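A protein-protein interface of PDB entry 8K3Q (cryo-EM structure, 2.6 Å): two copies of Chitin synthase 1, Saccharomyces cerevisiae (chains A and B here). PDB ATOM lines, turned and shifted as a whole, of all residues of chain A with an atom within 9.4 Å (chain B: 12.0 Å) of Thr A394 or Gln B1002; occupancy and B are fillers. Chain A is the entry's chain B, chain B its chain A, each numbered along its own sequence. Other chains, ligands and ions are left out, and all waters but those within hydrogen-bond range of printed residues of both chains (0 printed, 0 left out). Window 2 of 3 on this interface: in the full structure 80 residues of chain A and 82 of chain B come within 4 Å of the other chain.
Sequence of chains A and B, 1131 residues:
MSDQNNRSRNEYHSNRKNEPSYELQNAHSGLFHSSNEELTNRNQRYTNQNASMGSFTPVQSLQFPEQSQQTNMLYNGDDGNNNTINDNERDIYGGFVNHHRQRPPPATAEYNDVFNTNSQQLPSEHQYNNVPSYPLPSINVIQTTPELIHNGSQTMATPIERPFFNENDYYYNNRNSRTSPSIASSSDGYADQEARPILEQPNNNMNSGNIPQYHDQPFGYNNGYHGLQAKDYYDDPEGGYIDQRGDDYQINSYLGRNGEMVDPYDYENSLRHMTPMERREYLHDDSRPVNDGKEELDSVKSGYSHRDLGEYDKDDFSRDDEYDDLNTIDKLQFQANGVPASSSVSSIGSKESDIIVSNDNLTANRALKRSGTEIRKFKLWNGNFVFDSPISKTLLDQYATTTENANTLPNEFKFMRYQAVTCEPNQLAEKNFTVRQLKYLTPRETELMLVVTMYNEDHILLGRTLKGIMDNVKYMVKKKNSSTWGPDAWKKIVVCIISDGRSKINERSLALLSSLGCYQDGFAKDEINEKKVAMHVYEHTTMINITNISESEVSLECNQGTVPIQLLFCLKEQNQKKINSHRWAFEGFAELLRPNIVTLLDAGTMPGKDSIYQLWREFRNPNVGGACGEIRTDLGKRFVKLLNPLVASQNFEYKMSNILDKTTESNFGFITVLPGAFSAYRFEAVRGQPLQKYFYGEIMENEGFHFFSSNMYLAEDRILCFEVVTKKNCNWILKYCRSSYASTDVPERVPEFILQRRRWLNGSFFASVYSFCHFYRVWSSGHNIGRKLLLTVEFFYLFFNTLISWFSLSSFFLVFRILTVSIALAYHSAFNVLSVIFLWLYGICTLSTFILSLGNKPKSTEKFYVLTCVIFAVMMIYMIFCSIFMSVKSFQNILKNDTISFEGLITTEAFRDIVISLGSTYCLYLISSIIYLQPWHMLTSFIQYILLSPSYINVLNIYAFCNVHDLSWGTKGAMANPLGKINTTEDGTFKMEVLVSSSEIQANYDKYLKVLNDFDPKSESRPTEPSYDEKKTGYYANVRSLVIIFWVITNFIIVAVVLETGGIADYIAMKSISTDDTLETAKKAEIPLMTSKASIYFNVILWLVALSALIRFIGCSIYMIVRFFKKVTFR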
ATOM      1  N   TYR A 265      -4.538 -20.028  12.780  1.00  0.00           N
ATOM      2  CA  TYR A 265      -4.752 -21.036  11.748  1.00  0.00           C
ATOM      3  C   TYR A 265      -6.185 -21.543  11.764  1.00  0.00           C
ATOM      4  O   TYR A 265      -6.803 -21.714  10.707  1.00  0.00           O
ATOM      5  CB  TYR A 265      -3.781 -22.201  11.938  1.00  0.00           C
ATOM      6  CG  TYR A 265      -2.347 -21.860  11.626  1.00  0.00           C
ATOM      7  CD1 TYR A 265      -1.804 -22.107  10.377  1.00  0.00           C
ATOM      8  CD2 TYR A 265      -1.536 -21.293  12.587  1.00  0.00           C
ATOM      9  CE1 TYR A 265      -0.493 -21.795  10.103  1.00  0.00           C
ATOM     10  CE2 TYR A 265      -0.229 -20.982  12.320  1.00  0.00           C
ATOM     11  CZ  TYR A 265       0.288 -21.230  11.081  1.00  0.00           C
ATOM     12  OH  TYR A 265       1.598 -20.913  10.833  1.00  0.00           O
ATOM     13  N   PRO A 390       2.410 -17.148  14.075  1.00  0.00           N
ATOM     14  CA  PRO A 390       2.540 -18.072  12.951  1.00  0.00           C
ATOM     15  C   PRO A 390       3.698 -17.694  12.045  1.00  0.00           C
ATOM     16  O   PRO A 390       4.240 -16.591  12.100  1.00  0.00           O
ATOM     17  CB  PRO A 390       1.195 -17.926  12.230  1.00  0.00           C
ATOM     18  N   ILE A 391       4.100 -18.655  11.220  1.00  0.00           N
ATOM     19  CA  ILE A 391       5.184 -18.450  10.265  1.00  0.00           C
ATOM     20  C   ILE A 391       4.601 -18.201   8.881  1.00  0.00           C
ATOM     21  O   ILE A 391       3.428 -18.491   8.622  1.00  0.00           O
ATOM     22  CB  ILE A 391       6.147 -19.648  10.256  1.00  0.00           C
ATOM     23  CG1 ILE A 391       5.379 -20.937  10.006  1.00  0.00           C
ATOM     24  CG2 ILE A 391       6.884 -19.745  11.576  1.00  0.00           C
ATOM     25  CD1 ILE A 391       6.263 -22.112   9.772  1.00  0.00           C
ATOM     26  N   SER A 392       5.421 -17.658   7.986  1.00  0.00           N
ATOM     27  CA  SER A 392       5.004 -17.308   6.638  1.00  0.00           C
ATOM     28  C   SER A 392       4.746 -18.551   5.795  1.00  0.00           C
ATOM     29  O   SER A 392       5.428 -19.568   5.919  1.00  0.00           O
ATOM     30  CB  SER A 392       6.073 -16.454   5.982  1.00  0.00           C
ATOM     31  OG  SER A 392       7.246 -17.223   5.819  1.00  0.00           O
ATOM     32  N   LYS A 393       3.760 -18.450   4.895  1.00  0.00           N
ATOM     33  CA  LYS A 393       3.347 -19.615   4.120  1.00  0.00           C
ATOM     34  C   LYS A 393       4.446 -20.116   3.197  1.00  0.00           C
ATOM     35  O   LYS A 393       4.371 -21.256   2.720  1.00  0.00           O
ATOM     36  CB  LYS A 393       2.088 -19.301   3.310  1.00  0.00           C
ATOM     37  N   THR A 394       5.472 -19.300   2.949  1.00  0.00           N
ATOM     38  CA  THR A 394       6.597 -19.758   2.147  1.00  0.00           C
ATOM     39  C   THR A 394       7.258 -20.968   2.783  1.00  0.00           C
ATOM     40  O   THR A 394       7.600 -21.929   2.086  1.00  0.00           O
ATOM     41  CB  THR A 394       7.609 -18.632   1.968  1.00  0.00           C
ATOM     42  OG1 THR A 394       6.937 -17.476   1.467  1.00  0.00           O
ATOM     43  CG2 THR A 394       8.685 -19.040   0.976  1.00  0.00           C
ATOM     44  N   LEU A 395       7.434 -20.949   4.108  1.00  0.00           N
ATOM     45  CA  LEU A 395       7.936 -22.128   4.808  1.00  0.00           C
ATOM     46  C   LEU A 395       6.957 -23.289   4.722  1.00  0.00           C
ATOM     47  O   LEU A 395       7.369 -24.441   4.543  1.00  0.00           O
ATOM     48  CB  LEU A 395       8.233 -21.799   6.267  1.00  0.00           C
ATOM     49  CG  LEU A 395       9.404 -20.865   6.549  1.00  0.00           C
ATOM     50  CD1 LEU A 395       9.426 -20.476   8.009  1.00  0.00           C
ATOM     51  CD2 LEU A 395      10.697 -21.551   6.166  1.00  0.00           C
ATOM     52  N   LEU A 396       5.662 -23.010   4.854  1.00  0.00           N
ATOM     53  CA  LEU A 396       4.673 -24.077   4.802  1.00  0.00           C
ATOM     54  C   LEU A 396       4.716 -24.814   3.474  1.00  0.00           C
ATOM     55  O   LEU A 396       4.462 -26.025   3.425  1.00  0.00           O
ATOM     56  CB  LEU A 396       3.274 -23.514   5.040  1.00  0.00           C
ATOM     57  CG  LEU A 396       2.788 -23.391   6.484  1.00  0.00           C
ATOM     58  CD1 LEU A 396       2.769 -24.750   7.145  1.00  0.00           C
ATOM     59  CD2 LEU A 396       3.643 -22.424   7.266  1.00  0.00           C
ATOM     60  N   ASP A 397       5.040 -24.107   2.392  1.00  0.00           N
ATOM     61  CA  ASP A 397       5.103 -24.756   1.089  1.00  0.00           C
ATOM     62  C   ASP A 397       6.158 -25.857   1.066  1.00  0.00           C
ATOM     63  O   ASP A 397       5.913 -26.939   0.517  1.00  0.00           O
ATOM     64  CB  ASP A 397       5.370 -23.721  -0.002  1.00  0.00           C
ATOM     65  N   GLN A 398       7.336 -25.613   1.653  1.00  0.00           N
ATOM     66  CA  GLN A 398       8.296 -26.707   1.761  1.00  0.00           C
ATOM     67  C   GLN A 398       7.865 -27.734   2.793  1.00  0.00           C
ATOM     68  O   GLN A 398       8.052 -28.935   2.579  1.00  0.00           O
ATOM     69  CB  GLN A 398       9.697 -26.214   2.121  1.00  0.00           C
ATOM     70  CG  GLN A 398      10.413 -25.406   1.065  1.00  0.00           C
ATOM     71  CD  GLN A 398      10.126 -23.944   1.194  1.00  0.00           C
ATOM     72  OE1 GLN A 398       9.700 -23.489   2.248  1.00  0.00           O
ATOM     73  NE2 GLN A 398      10.361 -23.191   0.127  1.00  0.00           N
ATOM     74  N   TYR A 399       7.291 -27.284   3.911  1.00  0.00           N
ATOM     75  CA  TYR A 399       6.990 -28.198   5.008  1.00  0.00           C
ATOM     76  C   TYR A 399       6.003 -29.271   4.576  1.00  0.00           C
ATOM     77  O   TYR A 399       6.170 -30.450   4.911  1.00  0.00           O
ATOM     78  CB  TYR A 399       6.444 -27.421   6.202  1.00  0.00           C
ATOM     79  CG  TYR A 399       7.493 -26.703   7.014  1.00  0.00           C
ATOM     80  CD1 TYR A 399       8.807 -26.647   6.600  1.00  0.00           C
ATOM     81  CD2 TYR A 399       7.156 -26.050   8.183  1.00  0.00           C
ATOM     82  CE1 TYR A 399       9.756 -25.980   7.335  1.00  0.00           C
ATOM     83  CE2 TYR A 399       8.096 -25.381   8.918  1.00  0.00           C
ATOM     84  CZ  TYR A 399       9.392 -25.348   8.492  1.00  0.00           C
ATOM     85  OH  TYR A 399      10.332 -24.676   9.229  1.00  0.00           O
ATOM     86  N   ALA A 400       4.972 -28.886   3.822  1.00  0.00           N
ATOM     87  CA  ALA A 400       3.976 -29.859   3.391  1.00  0.00           C
ATOM     88  C   ALA A 400       4.597 -30.938   2.515  1.00  0.00           C
ATOM     89  O   ALA A 400       4.247 -32.117   2.628  1.00  0.00           O
ATOM     90  CB  ALA A 400       2.838 -29.156   2.655  1.00  0.00           C
ATOM     91  N   THR A 401       5.519 -30.557   1.639  1.00  0.00           N
ATOM     92  CA  THR A 401       6.205 -31.517   0.782  1.00  0.00           C
ATOM     93  C   THR A 401       7.100 -32.451   1.587  1.00  0.00           C
ATOM     94  O   THR A 401       7.246 -33.626   1.255  1.00  0.00           O
ATOM     95  CB  THR A 401       7.051 -30.807  -0.279  1.00  0.00           C
ATOM     96  OG1 THR A 401       8.052 -30.011   0.364  1.00  0.00           O
ATOM     97  CG2 THR A 401       6.177 -29.915  -1.135  1.00  0.00           C
ATOM     98  N   SER A 514      16.348 -15.824  11.019  1.00  0.00           N
ATOM     99  CA  SER A 514      14.972 -15.653  10.574  1.00  0.00           C
ATOM    100  C   SER A 514      14.634 -16.588   9.424  1.00  0.00           C
ATOM    101  O   SER A 514      13.519 -17.114   9.356  1.00  0.00           O
ATOM    102  CB  SER A 514      14.735 -14.214  10.155  1.00  0.00           C
ATOM    103  OG  SER A 514      13.433 -14.068   9.627  1.00  0.00           O
ATOM    104  N   SER A 515      15.567 -16.786   8.494  1.00  0.00           N
ATOM    105  CA  SER A 515      15.278 -17.636   7.345  1.00  0.00           C
ATOM    106  C   SER A 515      15.040 -19.079   7.767  1.00  0.00           C
ATOM    107  O   SER A 515      14.335 -19.826   7.082  1.00  0.00           O
ATOM    108  CB  SER A 515      16.414 -17.546   6.330  1.00  0.00           C
ATOM    109  OG  SER A 515      16.569 -16.216   5.876  1.00  0.00           O
ATOM    110  N   GLN A 520      11.293 -13.460  14.378  1.00  0.00           N
ATOM    111  CA  GLN A 520      10.451 -12.466  13.732  1.00  0.00           C
ATOM    112  C   GLN A 520      10.547 -11.212  14.577  1.00  0.00           C
ATOM    113  O   GLN A 520      10.467 -11.290  15.803  1.00  0.00           O
ATOM    114  CB  GLN A 520       8.993 -12.920  13.626  1.00  0.00           C
ATOM    115  CG  GLN A 520       8.781 -14.236  12.920  1.00  0.00           C
ATOM    116  CD  GLN A 520       7.326 -14.621  12.878  1.00  0.00           C
ATOM    117  OE1 GLN A 520       6.456 -13.803  13.154  1.00  0.00           O
ATOM    118  NE2 GLN A 520       7.051 -15.875  12.557  1.00  0.00           N
ATOM    119  N   ILE A 544      14.017 -27.121   7.681  1.00  0.00           N
ATOM    120  CA  ILE A 544      14.966 -26.779   6.630  1.00  0.00           C
ATOM    121  C   ILE A 544      16.385 -26.968   7.145  1.00  0.00           C
ATOM    122  O   ILE A 544      16.690 -26.715   8.314  1.00  0.00           O
ATOM    123  CB  ILE A 544      14.736 -25.347   6.102  1.00  0.00           C
ATOM    124  N   CYS A 558      14.759 -27.731   1.983  1.00  0.00           N
ATOM    125  CA  CYS A 558      13.835 -28.535   2.772  1.00  0.00           C
ATOM    126  C   CYS A 558      13.184 -29.561   1.863  1.00  0.00           C
ATOM    127  O   CYS A 558      12.517 -29.192   0.893  1.00  0.00           O
ATOM    128  CB  CYS A 558      12.762 -27.661   3.427  1.00  0.00           C
ATOM    129  SG  CYS A 558      11.667 -28.510   4.570  1.00  0.00           S
ATOM    130  N   VAL B 994       0.118  -5.478  16.617  1.00  0.00           N
ATOM    131  CA  VAL B 994       0.756  -6.723  16.215  1.00  0.00           C
ATOM    132  C   VAL B 994       0.560  -6.938  14.722  1.00  0.00           C
ATOM    133  O   VAL B 994      -0.510  -6.663  14.171  1.00  0.00           O
ATOM    134  CB  VAL B 994       0.201  -7.925  17.009  1.00  0.00           C
ATOM    135  N   LEU B 995       1.610  -7.423  14.062  1.00  0.00           N
ATOM    136  CA  LEU B 995       1.484  -7.878  12.683  1.00  0.00           C
ATOM    137  C   LEU B 995       0.575  -9.095  12.663  1.00  0.00           C
ATOM    138  O   LEU B 995       0.981 -10.190  13.065  1.00  0.00           O
ATOM    139  CB  LEU B 995       2.851  -8.211  12.094  1.00  0.00           C
ATOM    140  N   VAL B 996      -0.658  -8.910  12.206  1.00  0.00           N
ATOM    141  CA  VAL B 996      -1.646  -9.976  12.195  1.00  0.00           C
ATOM    142  C   VAL B 996      -1.830 -10.552  10.800  1.00  0.00           C
ATOM    143  O   VAL B 996      -1.909 -11.770  10.636  1.00  0.00           O
ATOM    144  CB  VAL B 996      -2.985  -9.470  12.768  1.00  0.00           C
ATOM    145  N   SER B 997      -1.900  -9.691   9.792  1.00  0.00           N
ATOM    146  CA  SER B 997      -2.112 -10.156   8.431  1.00  0.00           C
ATOM    147  C   SER B 997      -0.953 -11.034   7.982  1.00  0.00           C
ATOM    148  O   SER B 997       0.214 -10.735   8.245  1.00  0.00           O
ATOM    149  CB  SER B 997      -2.268  -8.967   7.484  1.00  0.00           C
ATOM    150  OG  SER B 997      -1.034  -8.296   7.316  1.00  0.00           O
ATOM    151  N   SER B 998      -1.289 -12.132   7.304  1.00  0.00           N
ATOM    152  CA  SER B 998      -0.265 -13.009   6.757  1.00  0.00           C
ATOM    153  C   SER B 998       0.664 -12.253   5.824  1.00  0.00           C
ATOM    154  O   SER B 998       1.861 -12.563   5.740  1.00  0.00           O
ATOM    155  CB  SER B 998      -0.925 -14.165   6.008  1.00  0.00           C
ATOM    156  N   SER B 999       0.130 -11.250   5.124  1.00  0.00           N
ATOM    157  CA  SER B 999       0.910 -10.521   4.134  1.00  0.00           C
ATOM    158  C   SER B 999       2.086  -9.800   4.775  1.00  0.00           C
ATOM    159  O   SER B 999       3.179  -9.762   4.204  1.00  0.00           O
ATOM    160  CB  SER B 999       0.014  -9.530   3.395  1.00  0.00           C
ATOM    161  OG  SER B 999      -0.696  -8.717   4.313  1.00  0.00           O
ATOM    162  N   GLU B1000       1.895  -9.240   5.968  1.00  0.00           N
ATOM    163  CA  GLU B1000       2.982  -8.499   6.596  1.00  0.00           C
ATOM    164  C   GLU B1000       4.037  -9.429   7.184  1.00  0.00           C
ATOM    165  O   GLU B1000       5.228  -9.096   7.191  1.00  0.00           O
ATOM    166  CB  GLU B1000       2.428  -7.565   7.665  1.00  0.00           C
ATOM    167  N   ILE B1001       3.625 -10.598   7.677  1.00  0.00           N
ATOM    168  CA  ILE B1001       4.597 -11.594   8.119  1.00  0.00           C
ATOM    169  C   ILE B1001       5.438 -12.063   6.943  1.00  0.00           C
ATOM    170  O   ILE B1001       6.667 -12.168   7.038  1.00  0.00           O
ATOM    171  CB  ILE B1001       3.878 -12.768   8.809  1.00  0.00           C
ATOM    172  CG1 ILE B1001       3.176 -12.282  10.076  1.00  0.00           C
ATOM    173  CG2 ILE B1001       4.860 -13.875   9.132  1.00  0.00           C
ATOM    174  CD1 ILE B1001       2.249 -13.298  10.687  1.00  0.00           C
ATOM    175  N   GLN B1002       4.788 -12.347   5.816  1.00  0.00           N
ATOM    176  CA  GLN B1002       5.515 -12.683   4.600  1.00  0.00           C
ATOM    177  C   GLN B1002       6.429 -11.541   4.168  1.00  0.00           C
ATOM    178  O   GLN B1002       7.538 -11.771   3.676  1.00  0.00           O
ATOM    179  CB  GLN B1002       4.513 -13.041   3.503  1.00  0.00           C
ATOM    180  CG  GLN B1002       5.080 -13.477   2.153  1.00  0.00           C
ATOM    181  CD  GLN B1002       5.866 -14.765   2.181  1.00  0.00           C
ATOM    182  OE1 GLN B1002       6.436 -15.147   3.194  1.00  0.00           O
ATOM    183  NE2 GLN B1002       5.866 -15.468   1.060  1.00  0.00           N
ATOM    184  N   ALA B1003       5.985 -10.299   4.355  1.00  0.00           N
ATOM    185  CA  ALA B1003       6.817  -9.157   3.994  1.00  0.00           C
ATOM    186  C   ALA B1003       8.092  -9.118   4.825  1.00  0.00           C
ATOM    187  O   ALA B1003       9.188  -8.938   4.285  1.00  0.00           O
ATOM    188  CB  ALA B1003       6.024  -7.863   4.165  1.00  0.00           C
ATOM    189  N   ASN B1004       7.967  -9.304   6.138  1.00  0.00           N
ATOM    190  CA  ASN B1004       9.137  -9.302   7.014  1.00  0.00           C
ATOM    191  C   ASN B1004      10.068 -10.469   6.686  1.00  0.00           C
ATOM    192  O   ASN B1004      11.300 -10.328   6.693  1.00  0.00           O
ATOM    193  CB  ASN B1004       8.673  -9.362   8.469  1.00  0.00           C
ATOM    194  N   TYR B1005       9.489 -11.635   6.395  1.00  0.00           N
ATOM    195  CA  TYR B1005      10.290 -12.793   6.023  1.00  0.00           C
ATOM    196  C   TYR B1005      11.053 -12.545   4.735  1.00  0.00           C
ATOM    197  O   TYR B1005      12.213 -12.942   4.604  1.00  0.00           O
ATOM    198  CB  TYR B1005       9.401 -14.025   5.890  1.00  0.00           C
ATOM    199  CG  TYR B1005      10.139 -15.261   5.442  1.00  0.00           C
ATOM    200  CD1 TYR B1005      10.019 -15.729   4.149  1.00  0.00           C
ATOM    201  CD2 TYR B1005      10.974 -15.945   6.308  1.00  0.00           C
ATOM    202  CE1 TYR B1005      10.686 -16.855   3.739  1.00  0.00           C
ATOM    203  CE2 TYR B1005      11.647 -17.066   5.907  1.00  0.00           C
ATOM    204  CZ  TYR B1005      11.504 -17.519   4.621  1.00  0.00           C
ATOM    205  OH  TYR B1005      12.181 -18.643   4.217  1.00  0.00           O
ATOM    206  N   ASP B1006      10.419 -11.894   3.764  1.00  0.00           N
ATOM    207  CA  ASP B1006      11.115 -11.588   2.520  1.00  0.00           C
ATOM    208  C   ASP B1006      12.188 -10.531   2.740  1.00  0.00           C
ATOM    209  O   ASP B1006      13.229 -10.546   2.076  1.00  0.00           O
ATOM    210  CB  ASP B1006      10.116 -11.140   1.457  1.00  0.00           C
ATOM    211  CG  ASP B1006       9.517 -12.307   0.695  1.00  0.00           C
ATOM    212  OD1 ASP B1006       8.744 -12.068  -0.257  1.00  0.00           O
ATOM    213  OD2 ASP B1006       9.820 -13.466   1.047  1.00  0.00           O
ATOM    214  N   LYS B1007      11.951  -9.600   3.665  1.00  0.00           N
ATOM    215  CA  LYS B1007      12.936  -8.557   3.928  1.00  0.00           C
ATOM    216  C   LYS B1007      14.184  -9.095   4.616  1.00  0.00           C
ATOM    217  O   LYS B1007      15.279  -8.585   4.365  1.00  0.00           O
ATOM    218  CB  LYS B1007      12.285  -7.421   4.721  1.00  0.00           C
ATOM    219  N   TYR B1008      14.050 -10.097   5.485  1.00  0.00           N
ATOM    220  CA  TYR B1008      15.204 -10.860   5.963  1.00  0.00           C
ATOM    221  C   TYR B1008      15.768 -11.875   4.982  1.00  0.00           C
ATOM    222  O   TYR B1008      16.963 -12.157   5.045  1.00  0.00           O
ATOM    223  CB  TYR B1008      14.883 -11.554   7.290  1.00  0.00           C
ATOM    224  CG  TYR B1008      14.753 -10.616   8.461  1.00  0.00           C
ATOM    225  CD1 TYR B1008      15.231  -9.329   8.388  1.00  0.00           C
ATOM    226  CD2 TYR B1008      14.088 -10.992   9.608  1.00  0.00           C
ATOM    227  CE1 TYR B1008      15.131  -8.475   9.456  1.00  0.00           C
ATOM    228  CE2 TYR B1008      13.960 -10.139  10.671  1.00  0.00           C
ATOM    229  CZ  TYR B1008      14.481  -8.877  10.590  1.00  0.00           C
ATOM    230  OH  TYR B1008      14.349  -8.011  11.649  1.00  0.00           O
ATOM    231  N   LEU B1009      14.973 -12.422   4.077  1.00  0.00           N
ATOM    232  CA  LEU B1009      15.532 -13.291   3.053  1.00  0.00           C
ATOM    233  C   LEU B1009      16.316 -12.504   2.011  1.00  0.00           C
ATOM    234  O   LEU B1009      17.158 -13.076   1.316  1.00  0.00           O
ATOM    235  CB  LEU B1009      14.406 -14.099   2.396  1.00  0.00           C
ATOM    236  CG  LEU B1009      14.673 -15.332   1.528  1.00  0.00           C
ATOM    237  CD1 LEU B1009      13.412 -16.166   1.454  1.00  0.00           C
ATOM    238  CD2 LEU B1009      15.105 -14.961   0.125  1.00  0.00           C
ATOM    239  N   LYS B1010      16.090 -11.195   1.931  1.00  0.00           N
ATOM    240  CA  LYS B1010      16.804 -10.310   1.024  1.00  0.00           C
ATOM    241  C   LYS B1010      18.206  -9.969   1.493  1.00  0.00           C
ATOM    242  O   LYS B1010      19.105  -9.840   0.660  1.00  0.00           O
ATOM    243  CB  LYS B1010      16.016  -9.007   0.837  1.00  0.00           C
ATOM    244  N   VAL B1011      18.412  -9.826   2.801  1.00  0.00           N
ATOM    245  CA  VAL B1011      19.730  -9.476   3.321  1.00  0.00           C
ATOM    246  C   VAL B1011      20.740 -10.566   2.986  1.00  0.00           C
ATOM    247  O   VAL B1011      21.931 -10.297   2.794  1.00  0.00           O
ATOM    248  CB  VAL B1011      19.647  -9.222   4.837  1.00  0.00           C
ATOM    249  CG1 VAL B1011      20.996  -8.824   5.389  1.00  0.00           C
ATOM    250  CG2 VAL B1011      18.608  -8.164   5.132  1.00  0.00           C
ATOM    251  N   ASN B1013      21.133 -12.063   0.288  1.00  0.00           N
ATOM    252  CA  ASN B1013      21.296 -12.139  -1.158  1.00  0.00           C
ATOM    253  C   ASN B1013      22.113 -10.980  -1.714  1.00  0.00           C
ATOM    254  O   ASN B1013      22.710 -11.098  -2.788  1.00  0.00           O
ATOM    255  CB  ASN B1013      19.933 -12.190  -1.852  1.00  0.00           C
ATOM    256  CG  ASN B1013      19.227 -13.513  -1.661  1.00  0.00           C
ATOM    257  OD1 ASN B1013      18.987 -13.948  -0.537  1.00  0.00           O
ATOM    258  ND2 ASN B1013      18.899 -14.171  -2.766  1.00  0.00           N
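The side-chain amide oxygen of Gln B1002 lies close to the side-chain hydroxyl of Ser A392 (3.4 Å).
OE1 of Gln B1002 sits at hydrogen-bond distance from OG1 of Thr A394 (2.9 Å).
O of Thr A394 sits close to OE1 of Gln A398, 2.6 Å away.
The backbone carbonyl oxygen (O) of Leu A395 lies close to the side-chain amide oxygen (OE1) of Gln A398.
Among the printed residues, pairs that only touch across the chains: Ser A392 with Ile B1001 (3.99 Å), Ser A392 with Tyr B1005 (3.5 Å), Thr A394 with Tyr B1005 (3.97 Å), Leu A395 with Tyr B1005 (3.8 Å), Ser A514 with Tyr B1005 (3.9 Å), Ser A514 with Tyr B1008 (3.1 Å) and Ser A515 with Tyr B1005 (3.8 Å).
Printed residues of chain B within 4 Å of Thr A394: Gln B1002 and Tyr B1005.
Of chain A, only Ser A392 and Thr A394 come within 4 Å of Gln B1002.
Of chain B, only Tyr B1005 (3.8 Å) comes within 4 Å of Leu A395.
No residue of chain B comes within 4 Å of Leu A396.
No residue of chain B comes within 4 Å of Gln A398.
No residue of chain A comes within 4 Å of Ala B1003.
No residue of chain A comes within 4 Å of Asn B1004.
Printed residues of chain A within 4 Å of Tyr B1008: Ser A514.
Of the printed residues of chain A, Ile B1001 touches Ser A392.
Printed residues of chain B within 4 Å of Ser A514: Tyr B1005 and Tyr B1008.
Lys B1007 touches none of the printed residues of chain A.
Ser B997 touches none of the printed residues of chain A.
The nearest residue of chain B that does not touch Thr A394 is Asp B1006 (5.0 Å).
The nearest residue of chain A that does not touch Gln B1002 is Lys A393 (4.6 Å).
The nearest printed residue of chain B that does not touch Ser A515 is Tyr B1008 (4.2 Å).
Of the 19 printed residues of chain B, 4 touch a printed residue of chain A.
Of the 18 printed residues of chain A, 5 touch a printed residue of chain B.
Printed residues of chain A that touch a printed residue of chain B: Ser A392, Thr A394, Leu A395, Ser A514 and Ser A515.
Hydrophobic or aromatic side chains of chain A that line the printed part of chain B: Leu A395.
Along chain A the printed residues that touch a printed residue of chain B span positions 392 to 515.
Among the printed residues, no Asp or Glu carboxylate lies within 4 Å of a Lys or Arg side-chain nitrogen of the other chain.
No position is printed for both chains.
Of the 9 pairs that touch across the chains among the printed residues, none has its exchanged pair printed and touching as well.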
